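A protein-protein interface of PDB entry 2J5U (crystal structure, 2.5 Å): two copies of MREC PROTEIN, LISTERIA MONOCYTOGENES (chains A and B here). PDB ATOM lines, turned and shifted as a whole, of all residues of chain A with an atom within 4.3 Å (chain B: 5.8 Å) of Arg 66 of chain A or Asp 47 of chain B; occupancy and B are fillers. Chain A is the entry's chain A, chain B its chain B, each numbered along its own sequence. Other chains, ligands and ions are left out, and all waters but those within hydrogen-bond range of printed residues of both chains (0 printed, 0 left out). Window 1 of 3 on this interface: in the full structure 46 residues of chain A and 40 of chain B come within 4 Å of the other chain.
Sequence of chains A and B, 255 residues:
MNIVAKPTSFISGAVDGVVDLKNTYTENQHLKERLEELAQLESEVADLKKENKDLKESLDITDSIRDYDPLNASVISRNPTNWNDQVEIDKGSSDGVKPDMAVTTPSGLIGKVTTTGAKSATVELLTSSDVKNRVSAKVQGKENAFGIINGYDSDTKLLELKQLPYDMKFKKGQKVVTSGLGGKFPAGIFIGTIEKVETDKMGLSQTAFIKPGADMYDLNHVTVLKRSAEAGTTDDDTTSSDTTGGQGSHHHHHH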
ATOM      1  N   SER A  64      16.126  24.905  19.376  1.00  0.00           N
ATOM      2  CA  SER A  64      14.901  24.532  20.060  1.00  0.00           C
ATOM      3  C   SER A  64      15.255  23.682  21.281  1.00  0.00           C
ATOM      4  O   SER A  64      16.400  23.269  21.466  1.00  0.00           O
ATOM      5  CB  SER A  64      13.984  23.738  19.136  1.00  0.00           C
ATOM      6  OG  SER A  64      14.409  22.394  19.057  1.00  0.00           O
ATOM      7  N   ILE A  65      14.248  23.412  22.096  1.00  0.00           N
ATOM      8  CA  ILE A  65      14.413  22.644  23.304  1.00  0.00           C
ATOM      9  C   ILE A  65      14.926  21.215  23.096  1.00  0.00           C
ATOM     10  O   ILE A  65      15.431  20.609  24.031  1.00  0.00           O
ATOM     11  CB  ILE A  65      13.075  22.616  24.074  1.00  0.00           C
ATOM     12  CG1 ILE A  65      13.300  22.984  25.542  1.00  0.00           C
ATOM     13  CG2 ILE A  65      12.403  21.268  23.913  1.00  0.00           C
ATOM     14  CD1 ILE A  65      14.208  22.072  26.275  1.00  0.00           C
ATOM     15  N   ARG A  66      14.831  20.665  21.888  1.00  0.00           N
ATOM     16  CA  ARG A  66      15.304  19.287  21.693  1.00  0.00           C
ATOM     17  C   ARG A  66      16.684  19.102  21.070  1.00  0.00           C
ATOM     18  O   ARG A  66      17.185  17.985  21.021  1.00  0.00           O
ATOM     19  CB  ARG A  66      14.311  18.492  20.852  1.00  0.00           C
ATOM     20  CG  ARG A  66      12.948  19.105  20.755  1.00  0.00           C
ATOM     21  CD  ARG A  66      12.029  18.217  19.947  1.00  0.00           C
ATOM     22  NE  ARG A  66      11.871  16.905  20.563  1.00  0.00           N
ATOM     23  CZ  ARG A  66      12.297  15.775  20.011  1.00  0.00           C
ATOM     24  NH1 ARG A  66      12.111  14.617  20.641  1.00  0.00           N
ATOM     25  NH2 ARG A  66      12.910  15.811  18.829  1.00  0.00           N
ATOM     26  N   ASP A  67      17.304  20.178  20.601  1.00  0.00           N
ATOM     27  CA  ASP A  67      18.606  20.060  19.956  1.00  0.00           C
ATOM     28  C   ASP A  67      19.774  19.816  20.905  1.00  0.00           C
ATOM     29  O   ASP A  67      19.734  20.215  22.066  1.00  0.00           O
ATOM     30  CB  ASP A  67      18.874  21.302  19.101  1.00  0.00           C
ATOM     31  CG  ASP A  67      17.851  21.469  17.987  1.00  0.00           C
ATOM     32  OD1 ASP A  67      17.465  20.436  17.396  1.00  0.00           O
ATOM     33  OD2 ASP A  67      17.434  22.618  17.697  1.00  0.00           O
ATOM     34  N   TYR A  68      20.817  19.157  20.405  1.00  0.00           N
ATOM     35  CA  TYR A  68      21.997  18.880  21.217  1.00  0.00           C
ATOM     36  C   TYR A  68      23.192  18.329  20.432  1.00  0.00           C
ATOM     37  O   TYR A  68      23.029  17.764  19.355  1.00  0.00           O
ATOM     38  CB  TYR A  68      21.640  17.892  22.330  1.00  0.00           C
ATOM     39  CG  TYR A  68      21.264  16.519  21.832  1.00  0.00           C
ATOM     40  CD1 TYR A  68      19.936  16.117  21.782  1.00  0.00           C
ATOM     41  CD2 TYR A  68      22.240  15.634  21.370  1.00  0.00           C
ATOM     42  CE1 TYR A  68      19.585  14.870  21.285  1.00  0.00           C
ATOM     43  CE2 TYR A  68      21.901  14.388  20.864  1.00  0.00           C
ATOM     44  CZ  TYR A  68      20.572  14.013  20.822  1.00  0.00           C
ATOM     45  OH  TYR A  68      20.227  12.796  20.281  1.00  0.00           O
ATOM     46  N   LYS A 138       8.487  14.328  31.321  1.00  0.00           N
ATOM     47  CA  LYS A 138       7.189  14.401  30.684  1.00  0.00           C
ATOM     48  C   LYS A 138       6.691  12.985  30.369  1.00  0.00           C
ATOM     49  O   LYS A 138       7.465  12.124  29.927  1.00  0.00           O
ATOM     50  CB  LYS A 138       7.294  15.207  29.389  1.00  0.00           C
ATOM     51  CG  LYS A 138       5.959  15.477  28.730  1.00  0.00           C
ATOM     52  CD  LYS A 138       6.128  16.291  27.471  1.00  0.00           C
ATOM     53  CE  LYS A 138       6.911  15.517  26.439  1.00  0.00           C
ATOM     54  NZ  LYS A 138       7.069  16.297  25.192  1.00  0.00           N
ATOM     55  N   GLN A 140       4.414  10.960  27.969  1.00  0.00           N
ATOM     56  CA  GLN A 140       3.733  11.101  26.690  1.00  0.00           C
ATOM     57  C   GLN A 140       2.353  10.467  26.719  1.00  0.00           C
ATOM     58  O   GLN A 140       2.174   9.359  27.220  1.00  0.00           O
ATOM     59  CB  GLN A 140       4.550  10.464  25.577  1.00  0.00           C
ATOM     60  CG  GLN A 140       5.951  10.985  25.476  1.00  0.00           C
ATOM     61  CD  GLN A 140       6.683  10.398  24.300  1.00  0.00           C
ATOM     62  OE1 GLN A 140       6.450   9.248  23.924  1.00  0.00           O
ATOM     63  NE2 GLN A 140       7.582  11.173  23.714  1.00  0.00           N
ATOM     64  N   VAL A 177       9.817  10.838  29.151  1.00  0.00           N
ATOM     65  CA  VAL A 177      10.996  11.446  28.547  1.00  0.00           C
ATOM     66  C   VAL A 177      11.387  12.712  29.288  1.00  0.00           C
ATOM     67  O   VAL A 177      10.653  13.185  30.143  1.00  0.00           O
ATOM     68  CB  VAL A 177      10.744  11.794  27.056  1.00  0.00           C
ATOM     69  CG1 VAL A 177      10.376  10.547  26.293  1.00  0.00           C
ATOM     70  CG2 VAL A 177       9.637  12.822  26.937  1.00  0.00           C
ATOM     71  N   PRO A 186      18.414  18.268  27.235  1.00  0.00           N
ATOM     72  CA  PRO A 186      17.632  18.576  26.040  1.00  0.00           C
ATOM     73  C   PRO A 186      16.362  17.779  26.305  1.00  0.00           C
ATOM     74  O   PRO A 186      16.390  16.828  27.088  1.00  0.00           O
ATOM     75  CB  PRO A 186      18.465  17.972  24.920  1.00  0.00           C
ATOM     76  CG  PRO A 186      19.113  16.813  25.587  1.00  0.00           C
ATOM     77  CD  PRO A 186      19.562  17.416  26.891  1.00  0.00           C
ATOM     78  N   ALA A 187      15.246  18.151  25.695  1.00  0.00           N
ATOM     79  CA  ALA A 187      14.030  17.392  25.938  1.00  0.00           C
ATOM     80  C   ALA A 187      13.938  16.214  24.971  1.00  0.00           C
ATOM     81  O   ALA A 187      14.592  16.202  23.932  1.00  0.00           O
ATOM     82  CB  ALA A 187      12.817  18.291  25.801  1.00  0.00           C
ATOM     83  N   GLY A 188      13.148  15.211  25.337  1.00  0.00           N
ATOM     84  CA  GLY A 188      12.979  14.071  24.463  1.00  0.00           C
ATOM     85  C   GLY A 188      13.839  12.849  24.714  1.00  0.00           C
ATOM     86  O   GLY A 188      13.705  11.858  24.003  1.00  0.00           O
ATOM     87  N   GLU B  42      10.188   5.247  19.265  1.00  0.00           N
ATOM     88  CA  GLU B  42       8.755   5.453  19.356  1.00  0.00           C
ATOM     89  C   GLU B  42       8.488   6.804  20.021  1.00  0.00           C
ATOM     90  O   GLU B  42       7.501   7.474  19.708  1.00  0.00           O
ATOM     91  CB  GLU B  42       8.117   4.330  20.167  1.00  0.00           C
ATOM     92  CG  GLU B  42       8.180   2.961  19.501  1.00  0.00           C
ATOM     93  CD  GLU B  42       7.566   1.861  20.359  1.00  0.00           C
ATOM     94  OE1 GLU B  42       6.417   2.025  20.829  1.00  0.00           O
ATOM     95  OE2 GLU B  42       8.231   0.827  20.569  1.00  0.00           O
ATOM     96  N   SER B  43       9.376   7.198  20.933  1.00  0.00           N
ATOM     97  CA  SER B  43       9.257   8.474  21.640  1.00  0.00           C
ATOM     98  C   SER B  43       9.555   9.638  20.719  1.00  0.00           C
ATOM     99  O   SER B  43       8.928  10.682  20.828  1.00  0.00           O
ATOM    100  CB  SER B  43      10.213   8.532  22.828  1.00  0.00           C
ATOM    101  OG  SER B  43       9.744   7.728  23.889  1.00  0.00           O
ATOM    102  N   GLU B  44      10.522   9.465  19.828  1.00  0.00           N
ATOM    103  CA  GLU B  44      10.867  10.522  18.888  1.00  0.00           C
ATOM    104  C   GLU B  44       9.677  10.789  17.976  1.00  0.00           C
ATOM    105  O   GLU B  44       9.349  11.940  17.666  1.00  0.00           O
ATOM    106  CB  GLU B  44      12.073  10.116  18.045  1.00  0.00           C
ATOM    107  CG  GLU B  44      13.366  10.031  18.829  1.00  0.00           C
ATOM    108  CD  GLU B  44      14.578   9.786  17.946  1.00  0.00           C
ATOM    109  OE1 GLU B  44      14.813  10.592  17.013  1.00  0.00           O
ATOM    110  OE2 GLU B  44      15.298   8.788  18.190  1.00  0.00           O
ATOM    111  N   VAL B  45       9.034   9.709  17.549  1.00  0.00           N
ATOM    112  CA  VAL B  45       7.878   9.807  16.681  1.00  0.00           C
ATOM    113  C   VAL B  45       6.804  10.651  17.358  1.00  0.00           C
ATOM    114  O   VAL B  45       6.407  11.694  16.838  1.00  0.00           O
ATOM    115  CB  VAL B  45       7.311   8.405  16.359  1.00  0.00           C
ATOM    116  CG1 VAL B  45       6.006   8.523  15.600  1.00  0.00           C
ATOM    117  CG2 VAL B  45       8.323   7.625  15.540  1.00  0.00           C
ATOM    118  N   ALA B  46       6.347  10.199  18.521  1.00  0.00           N
ATOM    119  CA  ALA B  46       5.314  10.905  19.263  1.00  0.00           C
ATOM    120  C   ALA B  46       5.644  12.383  19.472  1.00  0.00           C
ATOM    121  O   ALA B  46       4.805  13.248  19.215  1.00  0.00           O
ATOM    122  CB  ALA B  46       5.076  10.222  20.607  1.00  0.00           C
ATOM    123  N   ASP B  47       6.861  12.672  19.929  1.00  0.00           N
ATOM    124  CA  ASP B  47       7.273  14.051  20.173  1.00  0.00           C
ATOM    125  C   ASP B  47       7.327  14.892  18.909  1.00  0.00           C
ATOM    126  O   ASP B  47       6.901  16.046  18.912  1.00  0.00           O
ATOM    127  CB  ASP B  47       8.638  14.101  20.872  1.00  0.00           C
ATOM    128  CG  ASP B  47       8.526  14.162  22.399  1.00  0.00           C
ATOM    129  OD1 ASP B  47       9.579  14.271  23.066  1.00  0.00           O
ATOM    130  OD2 ASP B  47       7.398  14.103  22.937  1.00  0.00           O
ATOM    131  N   LEU B  48       7.857  14.330  17.829  1.00  0.00           N
ATOM    132  CA  LEU B  48       7.944  15.072  16.581  1.00  0.00           C
ATOM    133  C   LEU B  48       6.558  15.366  16.023  1.00  0.00           C
ATOM    134  O   LEU B  48       6.293  16.465  15.526  1.00  0.00           O
ATOM    135  CB  LEU B  48       8.771  14.288  15.574  1.00  0.00           C
ATOM    136  CG  LEU B  48      10.270  14.375  15.860  1.00  0.00           C
ATOM    137  CD1 LEU B  48      11.013  13.327  15.061  1.00  0.00           C
ATOM    138  CD2 LEU B  48      10.762  15.772  15.519  1.00  0.00           C
ATOM    139  N   LYS B  49       5.670  14.385  16.116  1.00  0.00           N
ATOM    140  CA  LYS B  49       4.318  14.566  15.629  1.00  0.00           C
ATOM    141  C   LYS B  49       3.698  15.789  16.281  1.00  0.00           C
ATOM    142  O   LYS B  49       3.273  16.717  15.592  1.00  0.00           O
ATOM    143  CB  LYS B  49       3.461  13.336  15.929  1.00  0.00           C
ATOM    144  CG  LYS B  49       3.663  12.191  14.950  1.00  0.00           C
ATOM    145  CD  LYS B  49       2.744  11.024  15.270  1.00  0.00           C
ATOM    146  CE  LYS B  49       2.919   9.900  14.260  1.00  0.00           C
ATOM    147  NZ  LYS B  49       2.028   8.742  14.553  1.00  0.00           N
ATOM    148  N   LYS B  50       3.656  15.803  17.610  1.00  0.00           N
ATOM    149  CA  LYS B  50       3.060  16.931  18.308  1.00  0.00           C
ATOM    150  C   LYS B  50       3.749  18.252  17.992  1.00  0.00           C
ATOM    151  O   LYS B  50       3.085  19.266  17.784  1.00  0.00           O
ATOM    152  CB  LYS B  50       3.052  16.697  19.822  1.00  0.00           C
ATOM    153  CG  LYS B  50       2.527  17.894  20.601  1.00  0.00           C
ATOM    154  CD  LYS B  50       2.285  17.589  22.070  1.00  0.00           C
ATOM    155  CE  LYS B  50       2.090  18.879  22.867  1.00  0.00           C
ATOM    156  NZ  LYS B  50       1.078  19.793  22.250  1.00  0.00           N
ATOM    157  N   GLU B  51       5.073  18.249  17.938  1.00  0.00           N
ATOM    158  CA  GLU B  51       5.789  19.484  17.657  1.00  0.00           C
ATOM    159  C   GLU B  51       5.544  19.969  16.228  1.00  0.00           C
ATOM    160  O   GLU B  51       5.538  21.175  15.956  1.00  0.00           O
ATOM    161  CB  GLU B  51       7.288  19.301  17.921  1.00  0.00           C
ATOM    162  CG  GLU B  51       8.072  20.597  17.892  1.00  0.00           C
ATOM    163  CD  GLU B  51       9.349  20.513  18.691  1.00  0.00           C
ATOM    164  OE1 GLU B  51       9.278  20.121  19.877  1.00  0.00           O
ATOM    165  OE2 GLU B  51      10.419  20.846  18.141  1.00  0.00           O
ATOM    166  N   ASN B  52       5.338  19.032  15.312  1.00  0.00           N
ATOM    167  CA  ASN B  52       5.085  19.415  13.937  1.00  0.00           C
ATOM    168  C   ASN B  52       3.689  20.027  13.812  1.00  0.00           C
ATOM    169  O   ASN B  52       3.514  21.081  13.195  1.00  0.00           O
ATOM    170  CB  ASN B  52       5.226  18.205  13.017  1.00  0.00           C
ATOM    171  CG  ASN B  52       6.664  17.750  12.881  1.00  0.00           C
ATOM    172  OD1 ASN B  52       7.571  18.566  12.747  1.00  0.00           O
ATOM    173  ND2 ASN B  52       6.875  16.445  12.897  1.00  0.00           N
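Asp 47 of chain B touches four residues of chain A.
Printed residues of chain A within 4 Å of Glu 51 of chain B: Arg 66 (3.3 Å).
Printed residues of chain A within 4 Å of Leu 48 of chain B: Arg 66 (3.9 Å).
Printed residues of chain B within 4 Å of Gly 188 of chain A: Asp 47 (3.7 Å).
Of the printed residues of chain B, Gln 140 of chain A touches Ser 43, Ala 46 and Asp 47.
The nearest residue of chain B that does not touch Arg 66 of chain A is Glu 44 of chain B (4.6 Å).
The nearest residue of chain A that does not touch Asp 47 of chain B is Val 177 of chain A (4.1 Å).
OD1 of Asp 47 of chain B lies within salt-bridge range of NH1 of Arg 66 of chain A (3.5 Å).
The side-chain amide nitrogen of Gln 140 of chain A lies within hydrogen-bond range of the backbone carbonyl oxygen of Ser 43 of chain B, 3.2 Å away.
NE2 of Gln 140 of chain A is in hydrogen-bond range of OD2 of Asp 47 of chain B (3.0 Å).
The side-chain amino group (NZ) of Lys 138 of chain A is in salt-bridge range of the side-chain carboxylate (OD2) of Asp 47 of chain B, 3.2 Å away.
The side-chain hydroxyl (OG) of Ser 64 of chain A lies close to the backbone NH (N) of Arg 66 of chain A (3.3 Å).
O of Leu 48 of chain B is in hydrogen-bond range of ND2 of Asn 52 of chain B, at 2.7 Å.
O of Val 177 of chain A is in hydrogen-bond range of N of Lys 138 of chain A, 2.7 Å away.
Of the 11 printed residues of chain B, 5 touch a printed residue of chain A.
Hydrophobic or aromatic side chains of chain B that line the printed part of chain A: Ala 46 and Leu 48.
Among the printed residues, Asp or Glu carboxylates within 4 Å of a Lys or Arg side-chain nitrogen of the other chain: Arg 66 of chain A with Asp 47 of chain B and Lys 138 of chain A with Asp 47 of chain B.
Among the printed residues, merely in contact across the chains: Arg 66 of chain A with Glu 51 of chain B (3.3 Å), Gly 188 of chain A with Asp 47 of chain B (3.7 Å), Gln 140 of chain A with Ala 46 of chain B (3.7 Å), Val 177 of chain A with Ser 43 of chain B (3.8 Å) and Arg 66 of chain A with Leu 48 of chain B (3.9 Å).
No position is printed for both chains.
Of the 9 pairs that touch across the chains among the printed residues, none has its exchanged pair printed and touching as well.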
